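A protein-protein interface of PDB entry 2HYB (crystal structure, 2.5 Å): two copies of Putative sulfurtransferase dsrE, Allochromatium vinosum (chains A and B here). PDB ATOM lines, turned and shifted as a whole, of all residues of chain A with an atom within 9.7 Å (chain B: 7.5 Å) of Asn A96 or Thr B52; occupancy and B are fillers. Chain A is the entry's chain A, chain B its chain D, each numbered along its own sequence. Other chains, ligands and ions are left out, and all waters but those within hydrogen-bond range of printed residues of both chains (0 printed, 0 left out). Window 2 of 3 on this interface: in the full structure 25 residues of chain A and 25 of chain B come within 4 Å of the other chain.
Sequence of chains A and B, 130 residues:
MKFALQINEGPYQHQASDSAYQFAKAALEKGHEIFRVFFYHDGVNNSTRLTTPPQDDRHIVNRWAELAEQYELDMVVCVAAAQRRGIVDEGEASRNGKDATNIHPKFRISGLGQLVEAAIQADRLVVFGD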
ATOM      1  N   VAL A  79      33.345  22.786 -22.842  1.00  0.00           N
ATOM      2  CA  VAL A  79      32.738  24.096 -23.021  1.00  0.00           C
ATOM      3  C   VAL A  79      33.109  24.727 -24.347  1.00  0.00           C
ATOM      4  O   VAL A  79      32.248  25.257 -25.049  1.00  0.00           O
ATOM      5  CB  VAL A  79      33.161  25.055 -21.906  1.00  0.00           C
ATOM      6  CG1 VAL A  79      34.675  25.146 -21.847  1.00  0.00           C
ATOM      7  CG2 VAL A  79      32.559  26.418 -22.152  1.00  0.00           C
ATOM      8  N   ALA A  80      34.388  24.678 -24.690  1.00  0.00           N
ATOM      9  CA  ALA A  80      34.853  25.264 -25.942  1.00  0.00           C
ATOM     10  C   ALA A  80      34.224  24.545 -27.126  1.00  0.00           C
ATOM     11  O   ALA A  80      33.844  25.165 -28.120  1.00  0.00           O
ATOM     12  CB  ALA A  80      36.377  25.182 -26.025  1.00  0.00           C
ATOM     13  N   ALA A  81      34.113  23.228 -27.010  1.00  0.00           N
ATOM     14  CA  ALA A  81      33.527  22.421 -28.067  1.00  0.00           C
ATOM     15  C   ALA A  81      32.061  22.798 -28.230  1.00  0.00           C
ATOM     16  O   ALA A  81      31.549  22.874 -29.345  1.00  0.00           O
ATOM     17  CB  ALA A  81      33.658  20.928 -27.720  1.00  0.00           C
ATOM     18  N   ALA A  82      31.408  23.051 -27.096  1.00  0.00           N
ATOM     19  CA  ALA A  82      29.995  23.413 -27.053  1.00  0.00           C
ATOM     20  C   ALA A  82      29.694  24.771 -27.668  1.00  0.00           C
ATOM     21  O   ALA A  82      28.716  24.929 -28.395  1.00  0.00           O
ATOM     22  CB  ALA A  82      29.508  23.376 -25.620  1.00  0.00           C
ATOM     23  N   GLN A  83      30.537  25.752 -27.376  1.00  0.00           N
ATOM     24  CA  GLN A  83      30.355  27.099 -27.909  1.00  0.00           C
ATOM     25  C   GLN A  83      30.416  27.097 -29.425  1.00  0.00           C
ATOM     26  O   GLN A  83      29.727  27.869 -30.086  1.00  0.00           O
ATOM     27  CB  GLN A  83      31.448  28.018 -27.387  1.00  0.00           C
ATOM     28  CG  GLN A  83      31.439  28.201 -25.896  1.00  0.00           C
ATOM     29  CD  GLN A  83      32.577  29.078 -25.441  1.00  0.00           C
ATOM     30  OE1 GLN A  83      32.619  29.505 -24.291  1.00  0.00           O
ATOM     31  NE2 GLN A  83      33.514  29.354 -26.347  1.00  0.00           N
ATOM     32  N   ARG A  84      31.259  26.229 -29.967  1.00  0.00           N
ATOM     33  CA  ARG A  84      31.441  26.130 -31.409  1.00  0.00           C
ATOM     34  C   ARG A  84      30.256  25.479 -32.133  1.00  0.00           C
ATOM     35  O   ARG A  84      29.844  25.923 -33.212  1.00  0.00           O
ATOM     36  CB  ARG A  84      32.730  25.346 -31.708  1.00  0.00           C
ATOM     37  CG  ARG A  84      33.551  25.952 -32.829  1.00  0.00           C
ATOM     38  CD  ARG A  84      34.909  25.293 -32.994  1.00  0.00           C
ATOM     39  NE  ARG A  84      35.623  25.157 -31.730  1.00  0.00           N
ATOM     40  CZ  ARG A  84      36.949  25.192 -31.622  1.00  0.00           C
ATOM     41  NH1 ARG A  84      37.704  25.367 -32.703  1.00  0.00           N
ATOM     42  NH2 ARG A  84      37.529  25.027 -30.438  1.00  0.00           N
ATOM     43  N   ARG A  85      29.699  24.444 -31.515  1.00  0.00           N
ATOM     44  CA  ARG A  85      28.604  23.690 -32.110  1.00  0.00           C
ATOM     45  C   ARG A  85      27.191  24.084 -31.711  1.00  0.00           C
ATOM     46  O   ARG A  85      26.246  23.805 -32.451  1.00  0.00           O
ATOM     47  CB  ARG A  85      28.834  22.206 -31.848  1.00  0.00           C
ATOM     48  CG  ARG A  85      30.147  21.740 -32.434  1.00  0.00           C
ATOM     49  CD  ARG A  85      30.567  20.383 -31.933  1.00  0.00           C
ATOM     50  NE  ARG A  85      31.803  19.973 -32.598  1.00  0.00           N
ATOM     51  CZ  ARG A  85      33.019  20.432 -32.307  1.00  0.00           C
ATOM     52  NH1 ARG A  85      33.185  21.322 -31.341  1.00  0.00           N
ATOM     53  NH2 ARG A  85      34.071  20.011 -32.996  1.00  0.00           N
ATOM     54  N   GLY A  86      27.030  24.722 -30.554  1.00  0.00           N
ATOM     55  CA  GLY A  86      25.695  25.138 -30.160  1.00  0.00           C
ATOM     56  C   GLY A  86      25.042  24.504 -28.945  1.00  0.00           C
ATOM     57  O   GLY A  86      23.813  24.487 -28.853  1.00  0.00           O
ATOM     58  N   ILE A  87      25.836  23.978 -28.015  1.00  0.00           N
ATOM     59  CA  ILE A  87      25.274  23.392 -26.800  1.00  0.00           C
ATOM     60  C   ILE A  87      25.324  24.489 -25.737  1.00  0.00           C
ATOM     61  O   ILE A  87      26.401  25.019 -25.438  1.00  0.00           O
ATOM     62  CB  ILE A  87      26.074  22.176 -26.342  1.00  0.00           C
ATOM     63  CG1 ILE A  87      25.985  21.077 -27.403  1.00  0.00           C
ATOM     64  CG2 ILE A  87      25.532  21.673 -25.014  1.00  0.00           C
ATOM     65  CD1 ILE A  87      24.583  20.550 -27.625  1.00  0.00           C
ATOM     66  N   VAL A  88      24.156  24.815 -25.176  1.00  0.00           N
ATOM     67  CA  VAL A  88      24.021  25.896 -24.201  1.00  0.00           C
ATOM     68  C   VAL A  88      23.255  25.572 -22.910  1.00  0.00           C
ATOM     69  O   VAL A  88      22.164  25.002 -22.943  1.00  0.00           O
ATOM     70  CB  VAL A  88      23.308  27.117 -24.865  1.00  0.00           C
ATOM     71  CG1 VAL A  88      23.223  28.283 -23.899  1.00  0.00           C
ATOM     72  CG2 VAL A  88      24.029  27.517 -26.142  1.00  0.00           C
ATOM     73  N   ASP A  89      23.834  25.954 -21.775  1.00  0.00           N
ATOM     74  CA  ASP A  89      23.183  25.760 -20.483  1.00  0.00           C
ATOM     75  C   ASP A  89      22.965  27.146 -19.857  1.00  0.00           C
ATOM     76  O   ASP A  89      23.307  28.168 -20.463  1.00  0.00           O
ATOM     77  CB  ASP A  89      24.042  24.899 -19.551  1.00  0.00           C
ATOM     78  CG  ASP A  89      25.365  25.558 -19.193  1.00  0.00           C
ATOM     79  OD1 ASP A  89      26.010  25.095 -18.227  1.00  0.00           O
ATOM     80  OD2 ASP A  89      25.754  26.533 -19.881  1.00  0.00           O
ATOM     81  N   GLU A  90      22.404  27.175 -18.651  1.00  0.00           N
ATOM     82  CA  GLU A  90      22.134  28.424 -17.936  1.00  0.00           C
ATOM     83  C   GLU A  90      23.318  29.403 -18.010  1.00  0.00           C
ATOM     84  O   GLU A  90      23.168  30.555 -18.420  1.00  0.00           O
ATOM     85  CB  GLU A  90      21.817  28.112 -16.469  1.00  0.00           C
ATOM     86  CG  GLU A  90      21.150  29.238 -15.697  1.00  0.00           C
ATOM     87  CD  GLU A  90      19.722  29.464 -16.133  1.00  0.00           C
ATOM     88  OE1 GLU A  90      19.047  30.323 -15.535  1.00  0.00           O
ATOM     89  OE2 GLU A  90      19.272  28.779 -17.075  1.00  0.00           O
ATOM     90  N   GLY A  91      24.492  28.931 -17.604  1.00  0.00           N
ATOM     91  CA  GLY A  91      25.679  29.768 -17.623  1.00  0.00           C
ATOM     92  C   GLY A  91      25.970  30.338 -18.994  1.00  0.00           C
ATOM     93  O   GLY A  91      25.975  31.550 -19.179  1.00  0.00           O
ATOM     94  N   GLU A  92      26.215  29.456 -19.957  1.00  0.00           N
ATOM     95  CA  GLU A  92      26.510  29.861 -21.327  1.00  0.00           C
ATOM     96  C   GLU A  92      25.489  30.844 -21.883  1.00  0.00           C
ATOM     97  O   GLU A  92      25.848  31.802 -22.567  1.00  0.00           O
ATOM     98  CB  GLU A  92      26.572  28.639 -22.249  1.00  0.00           C
ATOM     99  CG  GLU A  92      27.810  27.796 -22.084  1.00  0.00           C
ATOM    100  CD  GLU A  92      29.072  28.619 -22.178  1.00  0.00           C
ATOM    101  OE1 GLU A  92      29.526  29.135 -21.132  1.00  0.00           O
ATOM    102  OE2 GLU A  92      29.600  28.762 -23.299  1.00  0.00           O
ATOM    103  N   ALA A  93      24.214  30.589 -21.609  1.00  0.00           N
ATOM    104  CA  ALA A  93      23.144  31.454 -22.080  1.00  0.00           C
ATOM    105  C   ALA A  93      23.423  32.852 -21.546  1.00  0.00           C
ATOM    106  O   ALA A  93      23.403  33.839 -22.277  1.00  0.00           O
ATOM    107  CB  ALA A  93      21.801  30.949 -21.554  1.00  0.00           C
ATOM    108  N   SER A  94      23.709  32.898 -20.253  1.00  0.00           N
ATOM    109  CA  SER A  94      23.980  34.125 -19.532  1.00  0.00           C
ATOM    110  C   SER A  94      25.251  34.854 -19.982  1.00  0.00           C
ATOM    111  O   SER A  94      25.256  36.076 -20.127  1.00  0.00           O
ATOM    112  CB  SER A  94      24.050  33.793 -18.042  1.00  0.00           C
ATOM    113  OG  SER A  94      24.194  34.950 -17.255  1.00  0.00           O
ATOM    114  N   ARG A  95      26.322  34.113 -20.226  1.00  0.00           N
ATOM    115  CA  ARG A  95      27.582  34.731 -20.625  1.00  0.00           C
ATOM    116  C   ARG A  95      27.644  35.131 -22.085  1.00  0.00           C
ATOM    117  O   ARG A  95      28.282  36.118 -22.439  1.00  0.00           O
ATOM    118  CB  ARG A  95      28.726  33.784 -20.337  1.00  0.00           C
ATOM    119  CG  ARG A  95      28.524  33.010 -19.081  1.00  0.00           C
ATOM    120  CD  ARG A  95      29.696  32.129 -18.840  1.00  0.00           C
ATOM    121  NE  ARG A  95      30.919  32.909 -18.832  1.00  0.00           N
ATOM    122  CZ  ARG A  95      32.065  32.426 -18.386  1.00  0.00           C
ATOM    123  NH1 ARG A  95      32.100  31.184 -17.927  1.00  0.00           N
ATOM    124  NH2 ARG A  95      33.160  33.173 -18.396  1.00  0.00           N
ATOM    125  N   ASN A  96      26.968  34.365 -22.928  1.00  0.00           N
ATOM    126  CA  ASN A  96      26.995  34.611 -24.357  1.00  0.00           C
ATOM    127  C   ASN A  96      25.818  35.428 -24.872  1.00  0.00           C
ATOM    128  O   ASN A  96      25.801  35.840 -26.031  1.00  0.00           O
ATOM    129  CB  ASN A  96      27.069  33.273 -25.090  1.00  0.00           C
ATOM    130  CG  ASN A  96      28.255  32.427 -24.643  1.00  0.00           C
ATOM    131  OD1 ASN A  96      28.280  31.211 -24.851  1.00  0.00           O
ATOM    132  ND2 ASN A  96      29.248  33.070 -24.035  1.00  0.00           N
ATOM    133  N   GLY A  97      24.830  35.664 -24.020  1.00  0.00           N
ATOM    134  CA  GLY A  97      23.684  36.436 -24.452  1.00  0.00           C
ATOM    135  C   GLY A  97      22.838  35.682 -25.461  1.00  0.00           C
ATOM    136  O   GLY A  97      22.552  36.190 -26.546  1.00  0.00           O
ATOM    137  N   LYS A  98      22.432  34.467 -25.101  1.00  0.00           N
ATOM    138  CA  LYS A  98      21.609  33.635 -25.976  1.00  0.00           C
ATOM    139  C   LYS A  98      20.193  33.649 -25.429  1.00  0.00           C
ATOM    140  O   LYS A  98      19.999  33.651 -24.214  1.00  0.00           O
ATOM    141  CB  LYS A  98      22.130  32.197 -25.988  1.00  0.00           C
ATOM    142  CG  LYS A  98      23.633  32.063 -26.137  1.00  0.00           C
ATOM    143  CD  LYS A  98      24.039  31.829 -27.573  1.00  0.00           C
ATOM    144  CE  LYS A  98      23.808  33.050 -28.416  1.00  0.00           C
ATOM    145  NZ  LYS A  98      24.261  32.817 -29.798  1.00  0.00           N
ATOM    146  N   ASP A  99      19.210  33.636 -26.325  1.00  0.00           N
ATOM    147  CA  ASP A  99      17.805  33.660 -25.925  1.00  0.00           C
ATOM    148  C   ASP A  99      17.214  32.310 -25.495  1.00  0.00           C
ATOM    149  O   ASP A  99      15.996  32.195 -25.365  1.00  0.00           O
ATOM    150  CB  ASP A  99      16.948  34.247 -27.054  1.00  0.00           C
ATOM    151  CG  ASP A  99      17.006  33.416 -28.325  1.00  0.00           C
ATOM    152  OD1 ASP A  99      16.803  32.185 -28.248  1.00  0.00           O
ATOM    153  OD2 ASP A  99      17.242  33.986 -29.407  1.00  0.00           O
ATOM    154  N   ALA A 100      18.057  31.300 -25.272  1.00  0.00           N
ATOM    155  CA  ALA A 100      17.571  29.979 -24.855  1.00  0.00           C
ATOM    156  C   ALA A 100      18.692  28.998 -24.531  1.00  0.00           C
ATOM    157  O   ALA A 100      19.867  29.286 -24.759  1.00  0.00           O
ATOM    158  CB  ALA A 100      16.668  29.391 -25.933  1.00  0.00           C
ATOM    159  N   ILE A 109      28.461  21.211 -18.290  1.00  0.00           N
ATOM    160  CA  ILE A 109      29.458  21.812 -19.152  1.00  0.00           C
ATOM    161  C   ILE A 109      30.632  22.124 -18.255  1.00  0.00           C
ATOM    162  O   ILE A 109      30.447  22.492 -17.095  1.00  0.00           O
ATOM    163  CB  ILE A 109      28.934  23.106 -19.781  1.00  0.00           C
ATOM    164  CG1 ILE A 109      27.808  22.768 -20.756  1.00  0.00           C
ATOM    165  CG2 ILE A 109      30.080  23.857 -20.450  1.00  0.00           C
ATOM    166  CD1 ILE A 109      27.481  23.870 -21.745  1.00  0.00           C
ATOM    167  N   TYR B  12      32.366  23.066 -38.557  1.00  0.00           N
ATOM    168  CA  TYR B  12      33.688  22.928 -37.915  1.00  0.00           C
ATOM    169  C   TYR B  12      34.307  21.535 -37.830  1.00  0.00           C
ATOM    170  O   TYR B  12      35.519  21.379 -37.966  1.00  0.00           O
ATOM    171  CB  TYR B  12      33.674  23.538 -36.501  1.00  0.00           C
ATOM    172  CG  TYR B  12      33.261  24.992 -36.450  1.00  0.00           C
ATOM    173  CD1 TYR B  12      31.950  25.351 -36.124  1.00  0.00           C
ATOM    174  CD2 TYR B  12      34.166  26.011 -36.778  1.00  0.00           C
ATOM    175  CE1 TYR B  12      31.541  26.685 -36.128  1.00  0.00           C
ATOM    176  CE2 TYR B  12      33.769  27.354 -36.794  1.00  0.00           C
ATOM    177  CZ  TYR B  12      32.451  27.678 -36.469  1.00  0.00           C
ATOM    178  OH  TYR B  12      32.031  28.981 -36.522  1.00  0.00           O
ATOM    179  N   ARG B  49      21.088  28.740 -33.971  1.00  0.00           N
ATOM    180  CA  ARG B  49      21.441  30.123 -33.689  1.00  0.00           C
ATOM    181  C   ARG B  49      22.126  30.182 -32.338  1.00  0.00           C
ATOM    182  O   ARG B  49      22.390  31.260 -31.819  1.00  0.00           O
ATOM    183  CB  ARG B  49      20.184  30.993 -33.638  1.00  0.00           C
ATOM    184  CG  ARG B  49      19.192  30.568 -32.568  1.00  0.00           C
ATOM    185  CD  ARG B  49      18.189  31.674 -32.242  1.00  0.00           C
ATOM    186  NE  ARG B  49      17.371  31.359 -31.068  1.00  0.00           N
ATOM    187  CZ  ARG B  49      16.269  30.616 -31.100  1.00  0.00           C
ATOM    188  NH1 ARG B  49      15.835  30.105 -32.247  1.00  0.00           N
ATOM    189  NH2 ARG B  49      15.597  30.375 -29.986  1.00  0.00           N
ATOM    190  N   LEU B  50      22.427  29.023 -31.767  1.00  0.00           N
ATOM    191  CA  LEU B  50      23.052  28.995 -30.454  1.00  0.00           C
ATOM    192  C   LEU B  50      24.574  28.868 -30.405  1.00  0.00           C
ATOM    193  O   LEU B  50      25.134  28.605 -29.335  1.00  0.00           O
ATOM    194  CB  LEU B  50      22.426  27.874 -29.631  1.00  0.00           C
ATOM    195  CG  LEU B  50      20.910  27.965 -29.445  1.00  0.00           C
ATOM    196  CD1 LEU B  50      20.432  26.788 -28.606  1.00  0.00           C
ATOM    197  CD2 LEU B  50      20.546  29.293 -28.781  1.00  0.00           C
ATOM    198  N   THR B  51      25.254  29.059 -31.530  1.00  0.00           N
ATOM    199  CA  THR B  51      26.704  28.948 -31.502  1.00  0.00           C
ATOM    200  C   THR B  51      27.360  30.278 -31.128  1.00  0.00           C
ATOM    201  O   THR B  51      26.837  31.347 -31.428  1.00  0.00           O
ATOM    202  CB  THR B  51      27.283  28.454 -32.865  1.00  0.00           C
ATOM    203  OG1 THR B  51      27.210  29.494 -33.852  1.00  0.00           O
ATOM    204  CG2 THR B  51      26.522  27.236 -33.349  1.00  0.00           C
ATOM    205  N   THR B  52      28.506  30.180 -30.459  1.00  0.00           N
ATOM    206  CA  THR B  52      29.293  31.326 -30.039  1.00  0.00           C
ATOM    207  C   THR B  52      30.747  30.970 -30.331  1.00  0.00           C
ATOM    208  O   THR B  52      31.544  30.734 -29.425  1.00  0.00           O
ATOM    209  CB  THR B  52      29.107  31.598 -28.540  1.00  0.00           C
ATOM    210  OG1 THR B  52      27.708  31.707 -28.254  1.00  0.00           O
ATOM    211  CG2 THR B  52      29.795  32.890 -28.140  1.00  0.00           C
ATOM    212  N   PRO B  53      31.100  30.927 -31.621  1.00  0.00           N
ATOM    213  CA  PRO B  53      32.423  30.604 -32.156  1.00  0.00           C
ATOM    214  C   PRO B  53      33.500  31.612 -31.784  1.00  0.00           C
ATOM    215  O   PRO B  53      33.208  32.779 -31.521  1.00  0.00           O
ATOM    216  CB  PRO B  53      32.202  30.597 -33.672  1.00  0.00           C
ATOM    217  CG  PRO B  53      30.728  30.556 -33.849  1.00  0.00           C
ATOM    218  CD  PRO B  53      30.201  31.344 -32.703  1.00  0.00           C
ATOM    219  N   PRO B  54      34.763  31.161 -31.754  1.00  0.00           N
ATOM    220  CA  PRO B  54      35.897  32.024 -31.431  1.00  0.00           C
ATOM    221  C   PRO B  54      35.803  33.246 -32.339  1.00  0.00           C
ATOM    222  O   PRO B  54      35.587  33.116 -33.539  1.00  0.00           O
ATOM    223  CB  PRO B  54      37.086  31.135 -31.761  1.00  0.00           C
ATOM    224  CG  PRO B  54      36.593  29.794 -31.293  1.00  0.00           C
ATOM    225  CD  PRO B  54      35.189  29.751 -31.849  1.00  0.00           C
ATOM    226  N   GLN B  55      35.948  34.431 -31.765  1.00  0.00           N
ATOM    227  CA  GLN B  55      35.833  35.657 -32.540  1.00  0.00           C
ATOM    228  C   GLN B  55      36.932  35.847 -33.569  1.00  0.00           C
ATOM    229  O   GLN B  55      36.737  36.554 -34.562  1.00  0.00           O
ATOM    230  CB  GLN B  55      35.783  36.858 -31.602  1.00  0.00           C
ATOM    231  CG  GLN B  55      34.543  36.883 -30.730  1.00  0.00           C
ATOM    232  CD  GLN B  55      34.635  37.915 -29.628  1.00  0.00           C
ATOM    233  OE1 GLN B  55      34.811  39.104 -29.889  1.00  0.00           O
ATOM    234  NE2 GLN B  55      34.518  37.463 -28.384  1.00  0.00           N
ATOM    235  N   HIS B  59      32.439  32.618 -38.456  1.00  0.00           N
ATOM    236  CA  HIS B  59      31.206  32.201 -37.770  1.00  0.00           C
ATOM    237  C   HIS B  59      30.355  31.573 -38.872  1.00  0.00           C
ATOM    238  O   HIS B  59      29.559  32.245 -39.530  1.00  0.00           O
ATOM    239  CB  HIS B  59      30.496  33.431 -37.181  1.00  0.00           C
ATOM    240  CG  HIS B  59      29.355  33.114 -36.254  1.00  0.00           C
ATOM    241  ND1 HIS B  59      28.270  32.349 -36.626  1.00  0.00           N
ATOM    242  CD2 HIS B  59      29.099  33.529 -34.987  1.00  0.00           C
ATOM    243  CE1 HIS B  59      27.396  32.308 -35.633  1.00  0.00           C
ATOM    244  NE2 HIS B  59      27.876  33.019 -34.627  1.00  0.00           N
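The backbone carbonyl oxygen (O) of Gln A83 is in hydrogen-bond range of the backbone NH (N) of Thr B52, at 2.6 Å. The side-chain amide oxygen (OD1) of Asn A96 is in hydrogen-bond range of the side-chain hydroxyl (OG1) of Thr B52. NZ of Lys A98 sits at hydrogen-bond distance from O of Arg B49 (3.2 Å). The side-chain amino group (NZ) of Lys A98 is in hydrogen-bond range of the backbone carbonyl oxygen (O) of Thr B51 (3.4 Å). The side-chain carboxylate (OD1) of Asp A99 lies within salt-bridge range of the guanidinium group (NH2) of Arg B49, 2.8 Å away.
O of Ala A81 sits at hydrogen-bond distance from NH1 of Arg A85 (3.0 Å). OE1 of Gln A83 lies close to OE2 of Glu A92 (3.3 Å). The side-chain carboxylate (OE2) of Glu A92 lies close to the side-chain amide oxygen (OD1) of Asn A96 (3.2 Å). The backbone carbonyl oxygen (O) of Ala A93 lies within hydrogen-bond range of the backbone NH (N) of Lys A98.
Among the printed residues, pairs that only touch across the chains: Arg A84 with Tyr B12, Gln A83 with Thr B51, Val A88 with Leu B50, Arg A85 with Thr B51, Arg A84 with Thr B51, Gly A86 with Leu B50, Gln A83 with Pro B53, Lys A98 with Thr B52, Gly A86 with Thr B51 and Lys A98 with Leu B50.
Of the printed residues of chain B, Arg A84 touches Tyr B12 (3.5 Å) and Thr B51 (3.6 Å). Gly A91 touches none of the printed residues of chain B. Ser A94 touches none of the printed residues of chain B. Of the printed residues of chain B, Asn A96 touches Thr B52 (3.5 Å). No residue of chain B comes within 4 Å of Gly A97. Of the printed residues of chain B, Lys A98 touches Arg B49, Leu B50, Thr B51 and Thr B52. Of the printed residues of chain B, Asp A99 touches Arg B49. Of the printed residues of chain A, Arg B49 touches Lys A98 and Asp A99. Thr B51 touches just these residues of chain A: Gln A83 (3.5 Å), Arg A84 (3.6 Å), Arg A85 (3.6 Å), Gly A86 (3.8 Å) and Lys A98 (3.4 Å). Of the printed residues of chain A, Thr B52 touches Gln A83 (2.6 Å), Asn A96 (3.5 Å) and Lys A98 (3.7 Å). The nearest residue of chain A that does not touch Thr B52 is Arg A84 (4.5 Å).
Of the 23 printed residues of chain A, 8 touch a printed residue of chain B. Printed residues of chain A that touch a printed residue of chain B: Gln A83, Arg A84, Arg A85, Gly A86, Val A88, Asn A96, Lys A98 and Asp A99. Hydrophobic or aromatic side chains of chain A within 4 Å of the printed part of chain B: Val A88. Of the 9 printed residues of chain B, 6 touch a printed residue of chain A. Hydrophobic or aromatic side chains of chain B within 4 Å of the printed part of chain A: Tyr B12 and Leu B50. Among the printed residues, Asp or Glu carboxylates within 4 Å of a Lys or Arg side-chain nitrogen of the other chain: Asp A99 with Arg B49.
No position is printed for both chains. Of the 15 pairs that touch across the chains among the printed residues, none has its exchanged pair printed and touching as well.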
